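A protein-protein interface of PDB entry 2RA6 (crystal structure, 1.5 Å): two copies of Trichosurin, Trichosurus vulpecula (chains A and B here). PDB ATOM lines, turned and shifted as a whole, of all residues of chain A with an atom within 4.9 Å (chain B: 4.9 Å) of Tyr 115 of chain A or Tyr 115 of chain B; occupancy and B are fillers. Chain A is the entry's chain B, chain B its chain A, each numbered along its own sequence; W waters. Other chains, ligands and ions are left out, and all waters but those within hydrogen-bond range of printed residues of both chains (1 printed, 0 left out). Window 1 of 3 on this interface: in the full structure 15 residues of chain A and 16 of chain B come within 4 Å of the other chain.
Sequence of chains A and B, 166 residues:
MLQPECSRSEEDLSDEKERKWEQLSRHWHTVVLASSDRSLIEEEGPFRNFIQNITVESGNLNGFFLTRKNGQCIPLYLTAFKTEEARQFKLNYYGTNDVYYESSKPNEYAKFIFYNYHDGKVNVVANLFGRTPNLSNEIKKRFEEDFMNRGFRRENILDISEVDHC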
ATOM      1  N   THR A  96     -14.213  12.269 -15.415  1.00  0.00           N
ATOM      2  CA  THR A  96     -15.225  11.735 -14.514  1.00  0.00           C
ATOM      3  C   THR A  96     -14.831  12.083 -13.084  1.00  0.00           C
ATOM      4  O   THR A  96     -13.653  12.294 -12.796  1.00  0.00           O
ATOM      5  CB  THR A  96     -15.373  10.197 -14.650  1.00  0.00           C
ATOM      6  OG1 THR A  96     -14.149   9.554 -14.279  1.00  0.00           O
ATOM      7  CG2 THR A  96     -15.725   9.821 -16.084  1.00  0.00           C
ATOM      8  N   ASN A  97     -15.814  12.149 -12.190  1.00  0.00           N
ATOM      9  CA  ASN A  97     -15.540  12.501 -10.799  1.00  0.00           C
ATOM     10  C   ASN A  97     -16.353  11.705  -9.799  1.00  0.00           C
ATOM     11  O   ASN A  97     -17.539  11.445 -10.014  1.00  0.00           O
ATOM     12  CB  ASN A  97     -15.882  13.971 -10.535  1.00  0.00           C
ATOM     13  CG  ASN A  97     -15.192  14.919 -11.480  1.00  0.00           C
ATOM     14  OD1 ASN A  97     -14.092  15.402 -11.206  1.00  0.00           O
ATOM     15  ND2 ASN A  97     -15.842  15.205 -12.601  1.00  0.00           N
ATOM     16  N   ASP A  98     -15.708  11.303  -8.713  1.00  0.00           N
ATOM     17  CA  ASP A  98     -16.422  10.654  -7.627  1.00  0.00           C
ATOM     18  C   ASP A  98     -16.488  11.821  -6.653  1.00  0.00           C
ATOM     19  O   ASP A  98     -15.461  12.395  -6.287  1.00  0.00           O
ATOM     20  CB  ASP A  98     -15.634   9.487  -7.036  1.00  0.00           C
ATOM     21  CG  ASP A  98     -15.865   8.201  -7.800  1.00  0.00           C
ATOM     22  OD1 ASP A  98     -17.046   7.856  -8.039  1.00  0.00           O
ATOM     23  OD2 ASP A  98     -14.882   7.530  -8.154  1.00  0.00           O
ATOM     24  N   TYR A 100     -17.809  13.377  -2.966  1.00  0.00           N
ATOM     25  CA  TYR A 100     -18.251  13.033  -1.618  1.00  0.00           C
ATOM     26  C   TYR A 100     -18.644  14.283  -0.843  1.00  0.00           C
ATOM     27  O   TYR A 100     -17.919  15.275  -0.829  1.00  0.00           O
ATOM     28  CB  TYR A 100     -17.156  12.286  -0.848  1.00  0.00           C
ATOM     29  CG  TYR A 100     -16.843  10.905  -1.378  1.00  0.00           C
ATOM     30  CD1 TYR A 100     -15.950  10.728  -2.433  1.00  0.00           C
ATOM     31  CD2 TYR A 100     -17.443   9.777  -0.825  1.00  0.00           C
ATOM     32  CE1 TYR A 100     -15.662   9.455  -2.925  1.00  0.00           C
ATOM     33  CE2 TYR A 100     -17.165   8.504  -1.307  1.00  0.00           C
ATOM     34  CZ  TYR A 100     -16.275   8.348  -2.355  1.00  0.00           C
ATOM     35  OH  TYR A 100     -15.999   7.088  -2.835  1.00  0.00           O
ATOM     36  N   ILE A 113     -15.773  16.922  -1.724  1.00  0.00           N
ATOM     37  CA  ILE A 113     -14.473  16.442  -2.167  1.00  0.00           C
ATOM     38  C   ILE A 113     -14.673  15.776  -3.515  1.00  0.00           C
ATOM     39  O   ILE A 113     -15.493  14.867  -3.659  1.00  0.00           O
ATOM     40  CB  ILE A 113     -13.870  15.412  -1.194  1.00  0.00           C
ATOM     41  CG1 ILE A 113     -13.752  16.013   0.207  1.00  0.00           C
ATOM     42  CG2 ILE A 113     -12.501  14.961  -1.704  1.00  0.00           C
ATOM     43  CD1 ILE A 113     -12.882  17.250   0.286  1.00  0.00           C
ATOM     44  N   PHE A 114     -13.930  16.255  -4.504  1.00  0.00           N
ATOM     45  CA  PHE A 114     -13.987  15.717  -5.855  1.00  0.00           C
ATOM     46  C   PHE A 114     -12.754  14.895  -6.148  1.00  0.00           C
ATOM     47  O   PHE A 114     -11.635  15.375  -5.981  1.00  0.00           O
ATOM     48  CB  PHE A 114     -14.013  16.843  -6.887  1.00  0.00           C
ATOM     49  CG  PHE A 114     -15.336  17.513  -7.028  1.00  0.00           C
ATOM     50  CD1 PHE A 114     -16.121  17.281  -8.148  1.00  0.00           C
ATOM     51  CD2 PHE A 114     -15.806  18.371  -6.044  1.00  0.00           C
ATOM     52  CE1 PHE A 114     -17.359  17.893  -8.286  1.00  0.00           C
ATOM     53  CE2 PHE A 114     -17.043  18.987  -6.176  1.00  0.00           C
ATOM     54  CZ  PHE A 114     -17.817  18.747  -7.296  1.00  0.00           C
ATOM     55  N   TYR A 115     -12.958  13.658  -6.566  1.00  0.00           N
ATOM     56  CA  TYR A 115     -11.848  12.818  -6.977  1.00  0.00           C
ATOM     57  C   TYR A 115     -12.040  12.819  -8.485  1.00  0.00           C
ATOM     58  O   TYR A 115     -12.932  12.151  -9.016  1.00  0.00           O
ATOM     59  CB  TYR A 115     -11.975  11.412  -6.388  1.00  0.00           C
ATOM     60  CG  TYR A 115     -11.658  11.387  -4.910  1.00  0.00           C
ATOM     61  CD1 TYR A 115     -10.360  11.646  -4.458  1.00  0.00           C
ATOM     62  CD2 TYR A 115     -12.654  11.165  -3.963  1.00  0.00           C
ATOM     63  CE1 TYR A 115     -10.066  11.684  -3.099  1.00  0.00           C
ATOM     64  CE2 TYR A 115     -12.369  11.202  -2.597  1.00  0.00           C
ATOM     65  CZ  TYR A 115     -11.072  11.464  -2.179  1.00  0.00           C
ATOM     66  OH  TYR A 115     -10.777  11.511  -0.835  1.00  0.00           O
ATOM     67  N   ASN A 116     -11.213  13.610  -9.156  1.00  0.00           N
ATOM     68  CA  ASN A 116     -11.278  13.778 -10.600  1.00  0.00           C
ATOM     69  C   ASN A 116     -10.343  12.846 -11.351  1.00  0.00           C
ATOM     70  O   ASN A 116      -9.173  12.711 -11.002  1.00  0.00           O
ATOM     71  CB  ASN A 116     -10.961  15.242 -10.948  1.00  0.00           C
ATOM     72  CG  ASN A 116     -10.811  15.477 -12.443  1.00  0.00           C
ATOM     73  OD1 ASN A 116      -9.693  15.613 -12.949  1.00  0.00           O
ATOM     74  ND2 ASN A 116     -11.933  15.518 -13.158  1.00  0.00           N
ATOM     75  N   TYR A 117     -10.881  12.198 -12.379  1.00  0.00           N
ATOM     76  CA  TYR A 117     -10.114  11.283 -13.216  1.00  0.00           C
ATOM     77  C   TYR A 117     -10.066  11.938 -14.589  1.00  0.00           C
ATOM     78  O   TYR A 117     -11.079  12.012 -15.288  1.00  0.00           O
ATOM     79  CB  TYR A 117     -10.823   9.929 -13.289  1.00  0.00           C
ATOM     80  CG  TYR A 117     -11.210   9.390 -11.928  1.00  0.00           C
ATOM     81  CD1 TYR A 117     -10.236   9.025 -11.001  1.00  0.00           C
ATOM     82  CD2 TYR A 117     -12.549   9.269 -11.561  1.00  0.00           C
ATOM     83  CE1 TYR A 117     -10.589   8.551  -9.740  1.00  0.00           C
ATOM     84  CE2 TYR A 117     -12.912   8.795 -10.297  1.00  0.00           C
ATOM     85  CZ  TYR A 117     -11.921   8.440  -9.397  1.00  0.00           C
ATOM     86  OH  TYR A 117     -12.259   7.968  -8.151  1.00  0.00           O
ATOM     87  N   ASN A 123      -6.838  13.497  -9.433  1.00  0.00           N
ATOM     88  CA  ASN A 123      -6.577  14.710  -8.679  1.00  0.00           C
ATOM     89  C   ASN A 123      -7.690  14.887  -7.688  1.00  0.00           C
ATOM     90  O   ASN A 123      -8.785  14.360  -7.867  1.00  0.00           O
ATOM     91  CB  ASN A 123      -6.499  15.938  -9.577  1.00  0.00           C
ATOM     92  CG  ASN A 123      -5.087  16.200 -10.060  1.00  0.00           C
ATOM     93  OD1 ASN A 123      -4.166  16.461  -9.266  1.00  0.00           O
ATOM     94  ND2 ASN A 123      -4.904  16.131 -11.355  1.00  0.00           N
ATOM     95  N   VAL A 124      -7.399  15.603  -6.618  1.00  0.00           N
ATOM     96  CA  VAL A 124      -8.419  15.853  -5.627  1.00  0.00           C
ATOM     97  C   VAL A 124      -8.660  17.351  -5.577  1.00  0.00           C
ATOM     98  O   VAL A 124      -7.728  18.157  -5.591  1.00  0.00           O
ATOM     99  CB  VAL A 124      -8.003  15.332  -4.232  1.00  0.00           C
ATOM    100  CG1 VAL A 124      -6.772  16.071  -3.731  1.00  0.00           C
ATOM    101  CG2 VAL A 124      -9.161  15.498  -3.254  1.00  0.00           C
ATOM    102  N   THR B  96      -0.586   8.992   3.122  1.00  0.00           N
ATOM    103  CA  THR B  96      -1.857   8.957   3.829  1.00  0.00           C
ATOM    104  C   THR B  96      -2.907   8.422   2.870  1.00  0.00           C
ATOM    105  O   THR B  96      -2.744   8.518   1.654  1.00  0.00           O
ATOM    106  CB  THR B  96      -2.271  10.357   4.326  1.00  0.00           C
ATOM    107  OG1 THR B  96      -2.424  11.239   3.210  1.00  0.00           O
ATOM    108  CG2 THR B  96      -1.211  10.918   5.265  1.00  0.00           C
ATOM    109  N   ASN B  97      -3.977   7.850   3.410  1.00  0.00           N
ATOM    110  CA  ASN B  97      -5.032   7.292   2.571  1.00  0.00           C
ATOM    111  C   ASN B  97      -6.423   7.515   3.137  1.00  0.00           C
ATOM    112  O   ASN B  97      -6.649   7.369   4.338  1.00  0.00           O
ATOM    113  CB  ASN B  97      -4.873   5.775   2.420  1.00  0.00           C
ATOM    114  CG  ASN B  97      -3.510   5.366   1.938  1.00  0.00           C
ATOM    115  OD1 ASN B  97      -3.288   5.212   0.739  1.00  0.00           O
ATOM    116  ND2 ASN B  97      -2.578   5.174   2.874  1.00  0.00           N
ATOM    117  N   ASP B  98      -7.347   7.889   2.261  1.00  0.00           N
ATOM    118  CA  ASP B  98      -8.745   8.018   2.632  1.00  0.00           C
ATOM    119  C   ASP B  98      -9.302   6.701   2.096  1.00  0.00           C
ATOM    120  O   ASP B  98      -9.221   6.426   0.899  1.00  0.00           O
ATOM    121  CB  ASP B  98      -9.369   9.227   1.940  1.00  0.00           C
ATOM    122  CG  ASP B  98      -9.098  10.520   2.696  1.00  0.00           C
ATOM    123  OD1 ASP B  98      -8.991  11.587   2.064  1.00  0.00           O
ATOM    124  OD2 ASP B  98      -9.005  10.470   3.945  1.00  0.00           O
ATOM    125  N   TYR B 100     -12.483   3.973   1.644  1.00  0.00           N
ATOM    126  CA  TYR B 100     -13.937   3.834   1.598  1.00  0.00           C
ATOM    127  C   TYR B 100     -14.335   2.374   1.403  1.00  0.00           C
ATOM    128  O   TYR B 100     -13.821   1.692   0.518  1.00  0.00           O
ATOM    129  CB  TYR B 100     -14.522   4.664   0.452  1.00  0.00           C
ATOM    130  CG  TYR B 100     -14.387   6.150   0.648  1.00  0.00           C
ATOM    131  CD1 TYR B 100     -15.347   6.867   1.362  1.00  0.00           C
ATOM    132  CD2 TYR B 100     -13.296   6.838   0.124  1.00  0.00           C
ATOM    133  CE1 TYR B 100     -15.222   8.242   1.548  1.00  0.00           C
ATOM    134  CE2 TYR B 100     -13.156   8.212   0.302  1.00  0.00           C
ATOM    135  CZ  TYR B 100     -14.125   8.905   1.013  1.00  0.00           C
ATOM    136  OH  TYR B 100     -13.997  10.265   1.181  1.00  0.00           O
ATOM    137  N   ILE B 113     -11.836   1.092  -1.451  1.00  0.00           N
ATOM    138  CA  ILE B 113     -11.265   2.066  -2.364  1.00  0.00           C
ATOM    139  C   ILE B 113     -10.304   2.914  -1.539  1.00  0.00           C
ATOM    140  O   ILE B 113     -10.680   3.479  -0.508  1.00  0.00           O
ATOM    141  CB  ILE B 113     -12.351   2.977  -2.966  1.00  0.00           C
ATOM    142  CG1 ILE B 113     -13.421   2.130  -3.671  1.00  0.00           C
ATOM    143  CG2 ILE B 113     -11.716   3.974  -3.929  1.00  0.00           C
ATOM    144  CD1 ILE B 113     -12.873   1.118  -4.663  1.00  0.00           C
ATOM    145  N   PHE B 114      -9.060   2.972  -1.999  1.00  0.00           N
ATOM    146  CA  PHE B 114      -8.007   3.732  -1.346  1.00  0.00           C
ATOM    147  C   PHE B 114      -7.641   4.942  -2.178  1.00  0.00           C
ATOM    148  O   PHE B 114      -7.325   4.812  -3.358  1.00  0.00           O
ATOM    149  CB  PHE B 114      -6.739   2.887  -1.209  1.00  0.00           C
ATOM    150  CG  PHE B 114      -6.786   1.871  -0.111  1.00  0.00           C
ATOM    151  CD1 PHE B 114      -6.202   2.140   1.120  1.00  0.00           C
ATOM    152  CD2 PHE B 114      -7.398   0.641  -0.308  1.00  0.00           C
ATOM    153  CE1 PHE B 114      -6.224   1.197   2.144  1.00  0.00           C
ATOM    154  CE2 PHE B 114      -7.426  -0.313   0.712  1.00  0.00           C
ATOM    155  CZ  PHE B 114      -6.836  -0.029   1.938  1.00  0.00           C
ATOM    156  N   TYR B 115      -7.715   6.119  -1.575  1.00  0.00           N
ATOM    157  CA  TYR B 115      -7.288   7.326  -2.262  1.00  0.00           C
ATOM    158  C   TYR B 115      -5.972   7.598  -1.557  1.00  0.00           C
ATOM    159  O   TYR B 115      -5.949   8.000  -0.394  1.00  0.00           O
ATOM    160  CB  TYR B 115      -8.286   8.466  -2.070  1.00  0.00           C
ATOM    161  CG  TYR B 115      -9.517   8.272  -2.924  1.00  0.00           C
ATOM    162  CD1 TYR B 115     -10.743   7.928  -2.354  1.00  0.00           C
ATOM    163  CD2 TYR B 115      -9.434   8.361  -4.314  1.00  0.00           C
ATOM    164  CE1 TYR B 115     -11.860   7.672  -3.151  1.00  0.00           C
ATOM    165  CE2 TYR B 115     -10.539   8.107  -5.118  1.00  0.00           C
ATOM    166  CZ  TYR B 115     -11.743   7.763  -4.534  1.00  0.00           C
ATOM    167  OH  TYR B 115     -12.830   7.492  -5.334  1.00  0.00           O
ATOM    168  N   ASN B 116      -4.879   7.335  -2.261  1.00  0.00           N
ATOM    169  CA  ASN B 116      -3.550   7.496  -1.701  1.00  0.00           C
ATOM    170  C   ASN B 116      -2.906   8.822  -2.045  1.00  0.00           C
ATOM    171  O   ASN B 116      -2.964   9.272  -3.186  1.00  0.00           O
ATOM    172  CB  ASN B 116      -2.662   6.340  -2.172  1.00  0.00           C
ATOM    173  CG  ASN B 116      -1.209   6.516  -1.777  1.00  0.00           C
ATOM    174  OD1 ASN B 116      -0.376   6.879  -2.605  1.00  0.00           O
ATOM    175  ND2 ASN B 116      -0.898   6.266  -0.505  1.00  0.00           N
ATOM    176  N   TYR B 117      -2.317   9.455  -1.037  1.00  0.00           N
ATOM    177  CA  TYR B 117      -1.629  10.722  -1.236  1.00  0.00           C
ATOM    178  C   TYR B 117      -0.171  10.466  -0.878  1.00  0.00           C
ATOM    179  O   TYR B 117       0.162  10.222   0.283  1.00  0.00           O
ATOM    180  CB  TYR B 117      -2.210  11.813  -0.330  1.00  0.00           C
ATOM    181  CG  TYR B 117      -3.718  11.870  -0.321  1.00  0.00           C
ATOM    182  CD1 TYR B 117      -4.448  11.211   0.664  1.00  0.00           C
ATOM    183  CD2 TYR B 117      -4.419  12.566  -1.305  1.00  0.00           C
ATOM    184  CE1 TYR B 117      -5.837  11.240   0.674  1.00  0.00           C
ATOM    185  CE2 TYR B 117      -5.815  12.599  -1.306  1.00  0.00           C
ATOM    186  CZ  TYR B 117      -6.513  11.933  -0.310  1.00  0.00           C
ATOM    187  OH  TYR B 117      -7.890  11.954  -0.286  1.00  0.00           O
ATOM    188  N   ASN B 123      -3.493   8.902  -6.075  1.00  0.00           N
ATOM    189  CA  ASN B 123      -3.785   7.713  -6.854  1.00  0.00           C
ATOM    190  C   ASN B 123      -4.928   6.978  -6.205  1.00  0.00           C
ATOM    191  O   ASN B 123      -5.170   7.126  -5.007  1.00  0.00           O
ATOM    192  CB  ASN B 123      -2.583   6.774  -6.945  1.00  0.00           C
ATOM    193  CG  ASN B 123      -1.596   7.206  -8.002  1.00  0.00           C
ATOM    194  OD1 ASN B 123      -0.490   7.650  -7.689  1.00  0.00           O
ATOM    195  ND2 ASN B 123      -1.994   7.084  -9.268  1.00  0.00           N
ATOM    196  N   VAL B 124      -5.644   6.201  -7.005  1.00  0.00           N
ATOM    197  CA  VAL B 124      -6.745   5.410  -6.482  1.00  0.00           C
ATOM    198  C   VAL B 124      -6.356   3.944  -6.602  1.00  0.00           C
ATOM    199  O   VAL B 124      -5.816   3.510  -7.622  1.00  0.00           O
ATOM    200  CB  VAL B 124      -8.067   5.670  -7.256  1.00  0.00           C
ATOM    201  CG1 VAL B 124      -7.940   5.230  -8.704  1.00  0.00           C
ATOM    202  CG2 VAL B 124      -9.215   4.920  -6.576  1.00  0.00           C
HETATM  203  O   HOH W   1     -12.088  11.931   1.352  1.00  0.00           O
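Asp 98 of chain A touches Tyr 115 of chain B, and with the chains exchanged Tyr 115 of chain A touches Asp 98 of chain B.
Tyr 100 of chain A touches its own counterpart, Tyr 100 of chain B.
Tyr 115 of chain A touches Tyr 100 of chain B, but with the chains exchanged Tyr 100 of chain A does not touch Tyr 115 of chain B (4.1 Å).
Tyr 115 of chain A touches Tyr 117 of chain B, and with the chains exchanged Tyr 117 of chain A touches Tyr 115 of chain B.
Of the 7 pairs that touch across the chains among the printed residues, 6 have their exchanged pair printed and touching as well.
The side-chain hydroxyl of Tyr 115 of chain B sits at hydrogen-bond distance from the side-chain carboxylate of Asp 98 of chain A, at 3.5 Å.
OH of Tyr 117 of chain A is in hydrogen-bond range of OH of Tyr 115 of chain B (2.9 Å).
The side-chain carboxylate of Asp 98 of chain B lies within hydrogen-bond range of the side-chain hydroxyl of Tyr 115 of chain A, 3.4 Å away.
OH of Tyr 117 of chain B is in hydrogen-bond range of OH of Tyr 115 of chain A, 3.0 Å away.
Of the 11 printed residues of chain B, 4 touch a printed residue of chain A.
Hydrophobic or aromatic side chains of chain B that line the printed part of chain A: Tyr 100, Tyr 115 and Tyr 117.
Of the 11 printed residues of chain A, 4 touch a printed residue of chain B.
Among the printed residues, no Asp or Glu carboxylate lies within 4 Å of a Lys or Arg side-chain nitrogen of the other chain.
Tyr 100 of chain A touches Tyr 100 of chain B (CE2 to CE1, 3.5 Å).
OH of Tyr 100 of chain B touches OH of Tyr 115 of chain A (3.998 Å).
Tyr 115 of chain B touches Tyr 115 of chain A (CD2 to CD1, 3.4 Å).
OD1 of Asp 98 of chain B lies within hydrogen-bond range of OH of Tyr 117 of chain B (2.6 Å).
The side-chain hydroxyl (OH) of Tyr 117 of chain A lies within hydrogen-bond range of the side-chain carboxylate (OD2) of Asp 98 of chain A (2.7 Å).
The backbone NH of Tyr 100 of chain A lies within hydrogen-bond range of the backbone carbonyl oxygen of Ile 113 of chain A (2.8 Å).
The backbone carbonyl oxygen (O) of Ile 113 of chain B is in hydrogen-bond range of the backbone NH (N) of Tyr 100 of chain B, 2.9 Å away.
N of Tyr 115 of chain B is in hydrogen-bond range of O of Asp 98 of chain B (2.9 Å).
N of Tyr 117 of chain B sits at hydrogen-bond distance from O of Thr 96 of chain B (2.9 Å).
Water W1 lies within hydrogen-bond range of OH of Tyr 100 of chain B (2.5 Å), OH of Tyr 115 of chain A (2.6 Å) and OD1 of Asp 98 of chain B (3.2 Å).
Of the printed residues of chain B, Tyr 115 of chain A touches Asp 98, Tyr 100, Tyr 115 and Tyr 117.
Tyr 115 of chain B touches just these residues of chain A: Asp 98 (3.5 Å), Tyr 115 (3.4 Å) and Tyr 117 (2.9 Å).
Printed residues of chain A within 4 Å of Tyr 117 of chain B: Tyr 115 (3.0 Å).
Printed residues of chain B within 4 Å of Tyr 117 of chain A: Tyr 115 (2.9 Å).
The nearest residue of chain A that does not touch Tyr 115 of chain B is Tyr 100 of chain A (4.1 Å).
The nearest printed residue of chain A that does not touch Tyr 117 of chain B is Val 124 of chain A (4.3 Å).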
